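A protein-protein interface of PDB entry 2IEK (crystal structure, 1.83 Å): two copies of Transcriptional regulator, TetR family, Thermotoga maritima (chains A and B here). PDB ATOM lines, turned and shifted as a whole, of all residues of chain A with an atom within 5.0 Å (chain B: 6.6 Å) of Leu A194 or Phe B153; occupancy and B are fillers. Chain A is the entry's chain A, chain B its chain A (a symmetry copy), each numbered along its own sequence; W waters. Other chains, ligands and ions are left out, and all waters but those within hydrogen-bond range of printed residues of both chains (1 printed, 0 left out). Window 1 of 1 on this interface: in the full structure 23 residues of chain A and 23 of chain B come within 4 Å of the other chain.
Of the 15 printed residues of chain B, 9 touch a printed residue of chain A. Of the 15 printed residues of chain A, 8 touch a printed residue of chain B. Printed residues of chain A that touch a printed residue of chain B: Phe A153, Phe A157, Met A190, Ile A193, Leu A194, Lys A196, Gly A197 and Met A198. Among the printed residues, 14 pairs touch across the chains. Among the printed residues, no Asp or Glu carboxylate lies within 4 Å of a Lys or Arg side-chain nitrogen of the other chain.
Among the printed residues, pairs that only touch across the chains: Phe A153 with Phe B157, Phe A153 with Leu B194, Phe A157 with Phe B153, Met A190 with Ile B149, Met A190 with Lys B152, Met A190 with Phe B153, Met A190 with Trp B156, Ile A193 with Gly B197, Ile A193 with Met B198, Leu A194 with Phe B153, Lys A196 with Gly B197, Gly A197 with Ile B193, Gly A197 with Gly B197 and Met A198 with Ile B193.
Water W1 bridges O of Gly B197 (2.8 Å) and O of Arg A192 (3.3 Å).
Phe A153 touches Phe B157, and with the chains exchanged Phe A157 touches Phe B153. Ile A193 touches Gly B197, and with the chains exchanged Gly A197 touches Ile B193. Ile A193 touches Met B198, and with the chains exchanged Met A198 touches Ile B193. Gly A197 touches its own counterpart, Gly B197. 8 positions are printed for both chains. Of the 14 pairs that touch across the chains among the printed residues, 9 have their exchanged pair printed and touching as well.
Of chain B, only Phe B153 (3.8 Å) comes within 4 Å of Leu A194. Phe B153 touches just these residues of chain A: Phe A157 (3.6 Å), Met A190 (3.4 Å) and Leu A194 (3.8 Å). Printed residues of chain A within 4 Å of Leu B194: Phe A153 (3.8 Å). Of the printed residues of chain B, Met A190 touches Ile B149 (3.98 Å), Lys B152 (3.8 Å), Phe B153 (3.4 Å) and Trp B156 (3.5 Å). Printed residues of chain A within 4 Å of Gly B197: Ile A193, Lys A196 and Gly A197. Of the printed residues of chain A, Ile B193 touches Gly A197 (3.3 Å) and Met A198 (3.8 Å). Phe A158 touches none of the printed residues of chain B. Arg A192 touches none of the printed residues of chain B. The nearest residue of chain B that does not touch Leu A194 is Ile B193 (5.0 Å). The nearest residue of chain A that does not touch Phe B153 is Phe A153 (4.1 Å). The nearest printed residue of chain A that does not touch Phe B157 is Phe A157 (4.3 Å).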
ATOM      1  N   PHE A  79      -8.837   4.025  24.081  1.00  0.00           N
ATOM      2  CA  PHE A  79     -10.074   3.304  24.485  1.00  0.00           C
ATOM      3  C   PHE A  79      -9.825   1.882  24.928  1.00  0.00           C
ATOM      4  O   PHE A  79     -10.393   1.456  25.957  1.00  0.00           O
ATOM      5  CB  PHE A  79     -11.090   3.376  23.376  1.00  0.00           C
ATOM      6  CG  PHE A  79     -11.492   4.797  23.093  1.00  0.00           C
ATOM      7  CD1 PHE A  79     -10.889   5.489  22.036  1.00  0.00           C
ATOM      8  CD2 PHE A  79     -12.339   5.458  23.968  1.00  0.00           C
ATOM      9  CE1 PHE A  79     -11.237   6.839  21.788  1.00  0.00           C
ATOM     10  CE2 PHE A  79     -12.667   6.796  23.742  1.00  0.00           C
ATOM     11  CZ  PHE A  79     -12.104   7.467  22.646  1.00  0.00           C
ATOM     12  N   PHE A 153     -15.857  14.828  29.173  1.00  0.00           N
ATOM     13  CA  PHE A 153     -16.896  13.785  29.072  1.00  0.00           C
ATOM     14  C   PHE A 153     -16.438  12.512  29.808  1.00  0.00           C
ATOM     15  O   PHE A 153     -17.182  11.925  30.627  1.00  0.00           O
ATOM     16  CB  PHE A 153     -17.155  13.453  27.630  1.00  0.00           C
ATOM     17  CG  PHE A 153     -18.329  12.508  27.432  1.00  0.00           C
ATOM     18  CD1 PHE A 153     -18.207  11.156  27.702  1.00  0.00           C
ATOM     19  CD2 PHE A 153     -19.557  12.995  27.024  1.00  0.00           C
ATOM     20  CE1 PHE A 153     -19.323  10.274  27.537  1.00  0.00           C
ATOM     21  CE2 PHE A 153     -20.664  12.116  26.806  1.00  0.00           C
ATOM     22  CZ  PHE A 153     -20.521  10.763  27.073  1.00  0.00           C
ATOM     23  N   LEU A 154     -15.217  12.112  29.555  1.00  0.00           N
ATOM     24  CA  LEU A 154     -14.649  10.888  30.220  1.00  0.00           C
ATOM     25  C   LEU A 154     -14.638  11.070  31.727  1.00  0.00           C
ATOM     26  O   LEU A 154     -15.101  10.199  32.460  1.00  0.00           O
ATOM     27  CB  LEU A 154     -13.236  10.627  29.726  1.00  0.00           C
ATOM     28  CG  LEU A 154     -13.098  10.121  28.314  1.00  0.00           C
ATOM     29  CD1 LEU A 154     -11.651  10.279  27.823  1.00  0.00           C
ATOM     30  CD2 LEU A 154     -13.636   8.605  28.219  1.00  0.00           C
ATOM     31  N   PHE A 157     -18.188  10.786  33.072  1.00  0.00           N
ATOM     32  CA  PHE A 157     -18.697   9.358  32.991  1.00  0.00           C
ATOM     33  C   PHE A 157     -18.022   8.490  34.036  1.00  0.00           C
ATOM     34  O   PHE A 157     -18.686   7.685  34.744  1.00  0.00           O
ATOM     35  CB  PHE A 157     -18.424   8.792  31.611  1.00  0.00           C
ATOM     36  CG  PHE A 157     -18.704   7.288  31.502  1.00  0.00           C
ATOM     37  CD1 PHE A 157     -20.006   6.833  31.530  1.00  0.00           C
ATOM     38  CD2 PHE A 157     -17.665   6.394  31.433  1.00  0.00           C
ATOM     39  CE1 PHE A 157     -20.255   5.413  31.464  1.00  0.00           C
ATOM     40  CE2 PHE A 157     -17.915   5.000  31.336  1.00  0.00           C
ATOM     41  CZ  PHE A 157     -19.190   4.555  31.361  1.00  0.00           C
ATOM     42  N   PHE A 158     -16.697   8.586  34.121  1.00  0.00           N
ATOM     43  CA  PHE A 158     -15.981   7.792  35.161  1.00  0.00           C
ATOM     44  C   PHE A 158     -16.380   8.142  36.581  1.00  0.00           C
ATOM     45  O   PHE A 158     -16.487   7.232  37.449  1.00  0.00           O
ATOM     46  CB  PHE A 158     -14.491   7.918  35.005  1.00  0.00           C
ATOM     47  CG  PHE A 158     -13.973   7.336  33.751  1.00  0.00           C
ATOM     48  CD1 PHE A 158     -14.637   6.261  33.136  1.00  0.00           C
ATOM     49  CD2 PHE A 158     -12.777   7.793  33.206  1.00  0.00           C
ATOM     50  CE1 PHE A 158     -14.141   5.696  31.958  1.00  0.00           C
ATOM     51  CE2 PHE A 158     -12.285   7.231  32.054  1.00  0.00           C
ATOM     52  CZ  PHE A 158     -12.954   6.182  31.430  1.00  0.00           C
ATOM     53  N   MET A 190     -19.567  -0.278  26.732  1.00  0.00           N
ATOM     54  CA  MET A 190     -19.577   1.168  27.030  1.00  0.00           C
ATOM     55  C   MET A 190     -18.342   1.826  26.473  1.00  0.00           C
ATOM     56  O   MET A 190     -18.444   2.915  25.921  1.00  0.00           O
ATOM     57  CB  MET A 190     -19.747   1.459  28.523  1.00  0.00           C
ATOM     58  CG  MET A 190     -21.175   1.089  29.033  1.00  0.00           C
ATOM     59  SD  MET A 190     -21.285   1.303  30.936  1.00  0.00           S
ATOM     60  CE  MET A 190     -23.076   0.358  31.248  1.00  0.00           C
ATOM     61  N   LEU A 191     -17.165   1.209  26.617  1.00  0.00           N
ATOM     62  CA  LEU A 191     -15.936   1.804  26.003  1.00  0.00           C
ATOM     63  C   LEU A 191     -16.014   1.855  24.475  1.00  0.00           C
ATOM     64  O   LEU A 191     -15.436   2.737  23.838  1.00  0.00           O
ATOM     65  CB  LEU A 191     -14.681   1.079  26.530  1.00  0.00           C
ATOM     66  CG  LEU A 191     -13.961   1.708  27.752  1.00  0.00           C
ATOM     67  CD1 LEU A 191     -13.280   3.049  27.362  1.00  0.00           C
ATOM     68  CD2 LEU A 191     -14.912   1.985  28.932  1.00  0.00           C
ATOM     69  N   ARG A 192     -16.731   0.915  23.855  1.00  0.00           N
ATOM     70  CA  ARG A 192     -16.935   0.968  22.413  1.00  0.00           C
ATOM     71  C   ARG A 192     -17.924   2.067  22.026  1.00  0.00           C
ATOM     72  O   ARG A 192     -17.769   2.708  20.981  1.00  0.00           O
ATOM     73  CB  ARG A 192     -17.384  -0.407  21.871  1.00  0.00           C
ATOM     74  CG  ARG A 192     -16.200  -1.386  21.647  1.00  0.00           C
ATOM     75  CD  ARG A 192     -16.766  -2.740  20.982  1.00  0.00           C
ATOM     76  NE  ARG A 192     -17.148  -2.599  19.573  1.00  0.00           N
ATOM     77  CZ  ARG A 192     -18.398  -2.384  19.150  1.00  0.00           C
ATOM     78  NH1 ARG A 192     -19.401  -2.322  20.030  1.00  0.00           N
ATOM     79  NH2 ARG A 192     -18.650  -2.242  17.851  1.00  0.00           N
ATOM     80  N   ILE A 193     -18.879   2.378  22.906  1.00  0.00           N
ATOM     81  CA  ILE A 193     -19.796   3.505  22.655  1.00  0.00           C
ATOM     82  C   ILE A 193     -18.954   4.806  22.750  1.00  0.00           C
ATOM     83  O   ILE A 193     -19.149   5.706  21.910  1.00  0.00           O
ATOM     84  CB  ILE A 193     -20.894   3.603  23.744  1.00  0.00           C
ATOM     85  CG1 ILE A 193     -21.935   2.473  23.540  1.00  0.00           C
ATOM     86  CG2 ILE A 193     -21.571   4.989  23.716  1.00  0.00           C
ATOM     87  CD1 ILE A 193     -22.922   2.254  24.784  1.00  0.00           C
ATOM     88  N   LEU A 194     -18.121   4.911  23.781  1.00  0.00           N
ATOM     89  CA  LEU A 194     -17.231   6.161  23.894  1.00  0.00           C
ATOM     90  C   LEU A 194     -16.336   6.279  22.644  1.00  0.00           C
ATOM     91  O   LEU A 194     -16.199   7.352  22.012  1.00  0.00           O
ATOM     92  CB  LEU A 194     -16.366   6.037  25.161  1.00  0.00           C
ATOM     93  CG  LEU A 194     -17.077   6.206  26.524  1.00  0.00           C
ATOM     94  CD1 LEU A 194     -16.188   5.690  27.689  1.00  0.00           C
ATOM     95  CD2 LEU A 194     -17.451   7.661  26.682  1.00  0.00           C
ATOM     96  N   LYS A 195     -15.721   5.179  22.221  1.00  0.00           N
ATOM     97  CA  LYS A 195     -14.869   5.241  20.996  1.00  0.00           C
ATOM     98  C   LYS A 195     -15.620   5.707  19.741  1.00  0.00           C
ATOM     99  O   LYS A 195     -15.138   6.572  18.971  1.00  0.00           O
ATOM    100  CB  LYS A 195     -14.243   3.866  20.738  1.00  0.00           C
ATOM    101  CG  LYS A 195     -13.451   3.732  19.439  1.00  0.00           C
ATOM    102  CD  LYS A 195     -12.734   2.359  19.376  1.00  0.00           C
ATOM    103  CE  LYS A 195     -11.876   2.257  18.113  1.00  0.00           C
ATOM    104  NZ  LYS A 195     -11.452   0.857  17.851  1.00  0.00           N
ATOM    105  N   LYS A 196     -16.781   5.093  19.503  1.00  0.00           N
ATOM    106  CA  LYS A 196     -17.573   5.366  18.329  1.00  0.00           C
ATOM    107  C   LYS A 196     -18.116   6.832  18.378  1.00  0.00           C
ATOM    108  O   LYS A 196     -18.195   7.494  17.346  1.00  0.00           O
ATOM    109  CB  LYS A 196     -18.724   4.347  18.249  1.00  0.00           C
ATOM    110  CG  LYS A 196     -19.464   4.437  16.909  1.00  0.00           C
ATOM    111  CD  LYS A 196     -20.694   3.587  16.801  1.00  0.00           C
ATOM    112  CE  LYS A 196     -21.314   3.905  15.462  1.00  0.00           C
ATOM    113  NZ  LYS A 196     -22.318   2.929  15.130  1.00  0.00           N
ATOM    114  N   GLY A 197     -18.471   7.319  19.563  1.00  0.00           N
ATOM    115  CA  GLY A 197     -19.113   8.670  19.640  1.00  0.00           C
ATOM    116  C   GLY A 197     -18.087   9.784  19.608  1.00  0.00           C
ATOM    117  O   GLY A 197     -18.419  10.969  19.199  1.00  0.00           O
ATOM    118  N   MET A 198     -16.857   9.455  20.019  1.00  0.00           N
ATOM    119  CA  MET A 198     -15.798  10.515  20.099  1.00  0.00           C
ATOM    120  C   MET A 198     -14.864  10.610  18.894  1.00  0.00           C
ATOM    121  O   MET A 198     -14.146  11.615  18.715  1.00  0.00           O
ATOM    122  CB  MET A 198     -14.996  10.373  21.387  1.00  0.00           C
ATOM    123  CG  MET A 198     -15.772  10.667  22.654  1.00  0.00           C
ATOM    124  SD  MET A 198     -14.621  10.336  24.213  1.00  0.00           S
ATOM    125  CE  MET A 198     -12.981  11.194  23.538  1.00  0.00           C
ATOM    126  N   THR A 199     -14.861   9.589  18.031  1.00  0.00           N
ATOM    127  CA  THR A 199     -13.948   9.571  16.901  1.00  0.00           C
ATOM    128  C   THR A 199     -14.708   9.537  15.574  1.00  0.00           C
ATOM    129  O   THR A 199     -15.875   9.146  15.510  1.00  0.00           O
ATOM    130  CB  THR A 199     -12.926   8.375  17.005  1.00  0.00           C
ATOM    131  OG1 THR A 199     -13.629   7.155  16.770  1.00  0.00           O
ATOM    132  CG2 THR A 199     -12.292   8.293  18.370  1.00  0.00           C
ATOM    133  N   GLU B 148     -30.738  -2.243  27.605  1.00  0.00           N
ATOM    134  CA  GLU B 148     -30.252  -2.194  28.995  1.00  0.00           C
ATOM    135  C   GLU B 148     -28.917  -1.474  29.173  1.00  0.00           C
ATOM    136  O   GLU B 148     -28.800  -0.625  30.075  1.00  0.00           O
ATOM    137  CB  GLU B 148     -30.140  -3.600  29.589  1.00  0.00           C
ATOM    138  CG  GLU B 148     -29.803  -3.640  31.048  1.00  0.00           C
ATOM    139  N   ILE B 149     -27.917  -1.802  28.353  1.00  0.00           N
ATOM    140  CA  ILE B 149     -26.605  -1.101  28.398  1.00  0.00           C
ATOM    141  C   ILE B 149     -26.763   0.403  28.088  1.00  0.00           C
ATOM    142  O   ILE B 149     -26.123   1.274  28.762  1.00  0.00           O
ATOM    143  CB  ILE B 149     -25.562  -1.776  27.505  1.00  0.00           C
ATOM    144  CG1 ILE B 149     -25.219  -3.137  28.108  1.00  0.00           C
ATOM    145  CG2 ILE B 149     -24.209  -1.037  27.566  1.00  0.00           C
ATOM    146  CD1 ILE B 149     -24.029  -3.772  27.459  1.00  0.00           C
ATOM    147  N   ALA B 150     -27.603   0.708  27.101  1.00  0.00           N
ATOM    148  CA  ALA B 150     -27.827   2.123  26.701  1.00  0.00           C
ATOM    149  C   ALA B 150     -28.409   2.906  27.879  1.00  0.00           C
ATOM    150  O   ALA B 150     -27.957   4.004  28.198  1.00  0.00           O
ATOM    151  CB  ALA B 150     -28.758   2.185  25.494  1.00  0.00           C
ATOM    152  N   LEU B 151     -29.389   2.310  28.587  1.00  0.00           N
ATOM    153  CA  LEU B 151     -30.023   3.006  29.694  1.00  0.00           C
ATOM    154  C   LEU B 151     -29.019   3.160  30.832  1.00  0.00           C
ATOM    155  O   LEU B 151     -28.916   4.215  31.448  1.00  0.00           O
ATOM    156  CB  LEU B 151     -31.323   2.256  30.165  1.00  0.00           C
ATOM    157  CG  LEU B 151     -32.207   2.918  31.241  1.00  0.00           C
ATOM    158  CD1 LEU B 151     -32.672   4.292  30.762  1.00  0.00           C
ATOM    159  CD2 LEU B 151     -33.442   2.056  31.514  1.00  0.00           C
ATOM    160  N   LYS B 152     -28.265   2.100  31.141  1.00  0.00           N
ATOM    161  CA  LYS B 152     -27.268   2.187  32.211  1.00  0.00           C
ATOM    162  C   LYS B 152     -26.189   3.190  31.923  1.00  0.00           C
ATOM    163  O   LYS B 152     -25.750   3.957  32.823  1.00  0.00           O
ATOM    164  CB  LYS B 152     -26.621   0.818  32.459  1.00  0.00           C
ATOM    165  CG  LYS B 152     -27.478  -0.027  33.351  1.00  0.00           C
ATOM    166  CD  LYS B 152     -26.724  -1.362  33.533  1.00  0.00           C
ATOM    167  CE  LYS B 152     -27.166  -2.131  34.765  1.00  0.00           C
ATOM    168  NZ  LYS B 152     -26.486  -3.454  34.617  1.00  0.00           N
ATOM    169  N   PHE B 153     -25.760   3.228  30.674  1.00  0.00           N
ATOM    170  CA  PHE B 153     -24.705   4.199  30.325  1.00  0.00           C
ATOM    171  C   PHE B 153     -25.198   5.633  30.598  1.00  0.00           C
ATOM    172  O   PHE B 153     -24.505   6.452  31.243  1.00  0.00           O
ATOM    173  CB  PHE B 153     -24.346   4.071  28.871  1.00  0.00           C
ATOM    174  CG  PHE B 153     -23.152   4.921  28.471  1.00  0.00           C
ATOM    175  CD1 PHE B 153     -23.277   6.289  28.300  1.00  0.00           C
ATOM    176  CD2 PHE B 153     -21.904   4.344  28.317  1.00  0.00           C
ATOM    177  CE1 PHE B 153     -22.143   7.089  27.945  1.00  0.00           C
ATOM    178  CE2 PHE B 153     -20.776   5.125  27.912  1.00  0.00           C
ATOM    179  CZ  PHE B 153     -20.922   6.493  27.738  1.00  0.00           C
ATOM    180  N   LEU B 154     -26.395   5.921  30.152  1.00  0.00           N
ATOM    181  CA  LEU B 154     -26.994   7.285  30.366  1.00  0.00           C
ATOM    182  C   LEU B 154     -27.108   7.578  31.851  1.00  0.00           C
ATOM    183  O   LEU B 154     -26.686   8.638  32.308  1.00  0.00           O
ATOM    184  CB  LEU B 154     -28.368   7.365  29.721  1.00  0.00           C
ATOM    185  CG  LEU B 154     -28.405   7.408  28.216  1.00  0.00           C
ATOM    186  CD1 LEU B 154     -29.816   7.090  27.702  1.00  0.00           C
ATOM    187  CD2 LEU B 154     -27.845   8.826  27.693  1.00  0.00           C
ATOM    188  N   MET B 155     -27.675   6.646  32.636  1.00  0.00           N
ATOM    189  CA  MET B 155     -27.791   6.816  34.068  1.00  0.00           C
ATOM    190  C   MET B 155     -26.457   7.181  34.721  1.00  0.00           C
ATOM    191  O   MET B 155     -26.365   8.168  35.505  1.00  0.00           O
ATOM    192  CB  MET B 155     -28.411   5.540  34.702  1.00  0.00           C
ATOM    193  CG  MET B 155     -29.879   5.447  34.390  1.00  0.00           C
ATOM    194  SD  MET B 155     -30.597   3.741  35.140  1.00  0.00           S
ATOM    195  CE  MET B 155     -32.511   4.028  34.940  1.00  0.00           C
ATOM    196  N   TRP B 156     -25.408   6.422  34.393  1.00  0.00           N
ATOM    197  CA  TRP B 156     -24.122   6.649  35.002  1.00  0.00           C
ATOM    198  C   TRP B 156     -23.544   8.008  34.560  1.00  0.00           C
ATOM    199  O   TRP B 156     -22.982   8.766  35.383  1.00  0.00           O
ATOM    200  CB  TRP B 156     -23.161   5.541  34.660  1.00  0.00           C
ATOM    201  CG  TRP B 156     -23.590   4.155  35.207  1.00  0.00           C
ATOM    202  CD1 TRP B 156     -24.730   3.828  35.872  1.00  0.00           C
ATOM    203  CD2 TRP B 156     -22.864   2.957  35.018  1.00  0.00           C
ATOM    204  NE1 TRP B 156     -24.757   2.423  36.128  1.00  0.00           N
ATOM    205  CE2 TRP B 156     -23.598   1.897  35.612  1.00  0.00           C
ATOM    206  CE3 TRP B 156     -21.656   2.677  34.401  1.00  0.00           C
ATOM    207  CZ2 TRP B 156     -23.131   0.592  35.605  1.00  0.00           C
ATOM    208  CZ3 TRP B 156     -21.173   1.379  34.410  1.00  0.00           C
ATOM    209  CH2 TRP B 156     -21.929   0.348  35.009  1.00  0.00           C
ATOM    210  N   PHE B 157     -23.654   8.303  33.278  1.00  0.00           N
ATOM    211  CA  PHE B 157     -23.126   9.640  32.793  1.00  0.00           C
ATOM    212  C   PHE B 157     -23.860  10.782  33.470  1.00  0.00           C
ATOM    213  O   PHE B 157     -23.237  11.774  33.937  1.00  0.00           O
ATOM    214  CB  PHE B 157     -23.299   9.749  31.290  1.00  0.00           C
ATOM    215  CG  PHE B 157     -22.996  11.148  30.741  1.00  0.00           C
ATOM    216  CD1 PHE B 157     -21.693  11.603  30.714  1.00  0.00           C
ATOM    217  CD2 PHE B 157     -24.019  11.966  30.329  1.00  0.00           C
ATOM    218  CE1 PHE B 157     -21.425  12.936  30.229  1.00  0.00           C
ATOM    219  CE2 PHE B 157     -23.747  13.264  29.822  1.00  0.00           C
ATOM    220  CZ  PHE B 157     -22.472  13.708  29.793  1.00  0.00           C
ATOM    221  N   PHE B 158     -25.188  10.703  33.492  1.00  0.00           N
ATOM    222  CA  PHE B 158     -25.965  11.772  34.183  1.00  0.00           C
ATOM    223  C   PHE B 158     -25.665  11.883  35.666  1.00  0.00           C
ATOM    224  O   PHE B 158     -25.607  13.019  36.215  1.00  0.00           O
ATOM    225  CB  PHE B 158     -27.441  11.588  33.974  1.00  0.00           C
ATOM    226  CG  PHE B 158     -27.868  11.748  32.569  1.00  0.00           C
ATOM    227  CD1 PHE B 158     -27.152  12.587  31.698  1.00  0.00           C
ATOM    228  CD2 PHE B 158     -29.029  11.132  32.114  1.00  0.00           C
ATOM    229  CE1 PHE B 158     -27.562  12.754  30.373  1.00  0.00           C
ATOM    230  CE2 PHE B 158     -29.436  11.304  30.814  1.00  0.00           C
ATOM    231  CZ  PHE B 158     -28.716  12.116  29.943  1.00  0.00           C
ATOM    232  N   ILE B 193     -22.189  13.157  21.079  1.00  0.00           N
ATOM    233  CA  ILE B 193     -21.269  12.018  21.252  1.00  0.00           C
ATOM    234  C   ILE B 193     -22.131  10.802  21.688  1.00  0.00           C
ATOM    235  O   ILE B 193     -21.889   9.688  21.183  1.00  0.00           O
ATOM    236  CB  ILE B 193     -20.249  12.274  22.389  1.00  0.00           C
ATOM    237  CG1 ILE B 193     -19.185  13.296  21.916  1.00  0.00           C
ATOM    238  CG2 ILE B 193     -19.587  10.955  22.837  1.00  0.00           C
ATOM    239  CD1 ILE B 193     -18.282  13.901  23.094  1.00  0.00           C
ATOM    240  N   LEU B 194     -23.032  11.012  22.642  1.00  0.00           N
ATOM    241  CA  LEU B 194     -23.941   9.849  23.076  1.00  0.00           C
ATOM    242  C   LEU B 194     -24.751   9.341  21.867  1.00  0.00           C
ATOM    243  O   LEU B 194     -24.856   8.123  21.590  1.00  0.00           O
ATOM    244  CB  LEU B 194     -24.888  10.350  24.182  1.00  0.00           C
ATOM    245  CG  LEU B 194     -24.272  10.619  25.575  1.00  0.00           C
ATOM    246  CD1 LEU B 194     -25.232  11.460  26.459  1.00  0.00           C
ATOM    247  CD2 LEU B 194     -23.925   9.288  26.200  1.00  0.00           C
ATOM    248  N   GLY B 197     -22.425   7.421  19.410  1.00  0.00           N
ATOM    249  CA  GLY B 197     -21.804   6.167  19.945  1.00  0.00           C
ATOM    250  C   GLY B 197     -22.837   5.087  20.190  1.00  0.00           C
ATOM    251  O   GLY B 197     -22.491   3.837  20.191  1.00  0.00           O
ATOM    252  N   MET B 198     -24.088   5.513  20.395  1.00  0.00           N
ATOM    253  CA  MET B 198     -25.162   4.519  20.728  1.00  0.00           C
ATOM    254  C   MET B 198     -26.013   4.046  19.552  1.00  0.00           C
ATOM    255  O   MET B 198     -26.728   3.027  19.644  1.00  0.00           O
ATOM    256  CB  MET B 198     -26.046   5.044  21.852  1.00  0.00           C
ATOM    257  CG  MET B 198     -25.361   5.166  23.197  1.00  0.00           C
ATOM    258  SD  MET B 198     -26.611   5.950  24.495  1.00  0.00           S
ATOM    259  CE  MET B 198     -28.211   4.908  24.010  1.00  0.00           C
HETATM  260  O   HOH W   1     -20.753   1.651  19.899  1.00  0.00           O
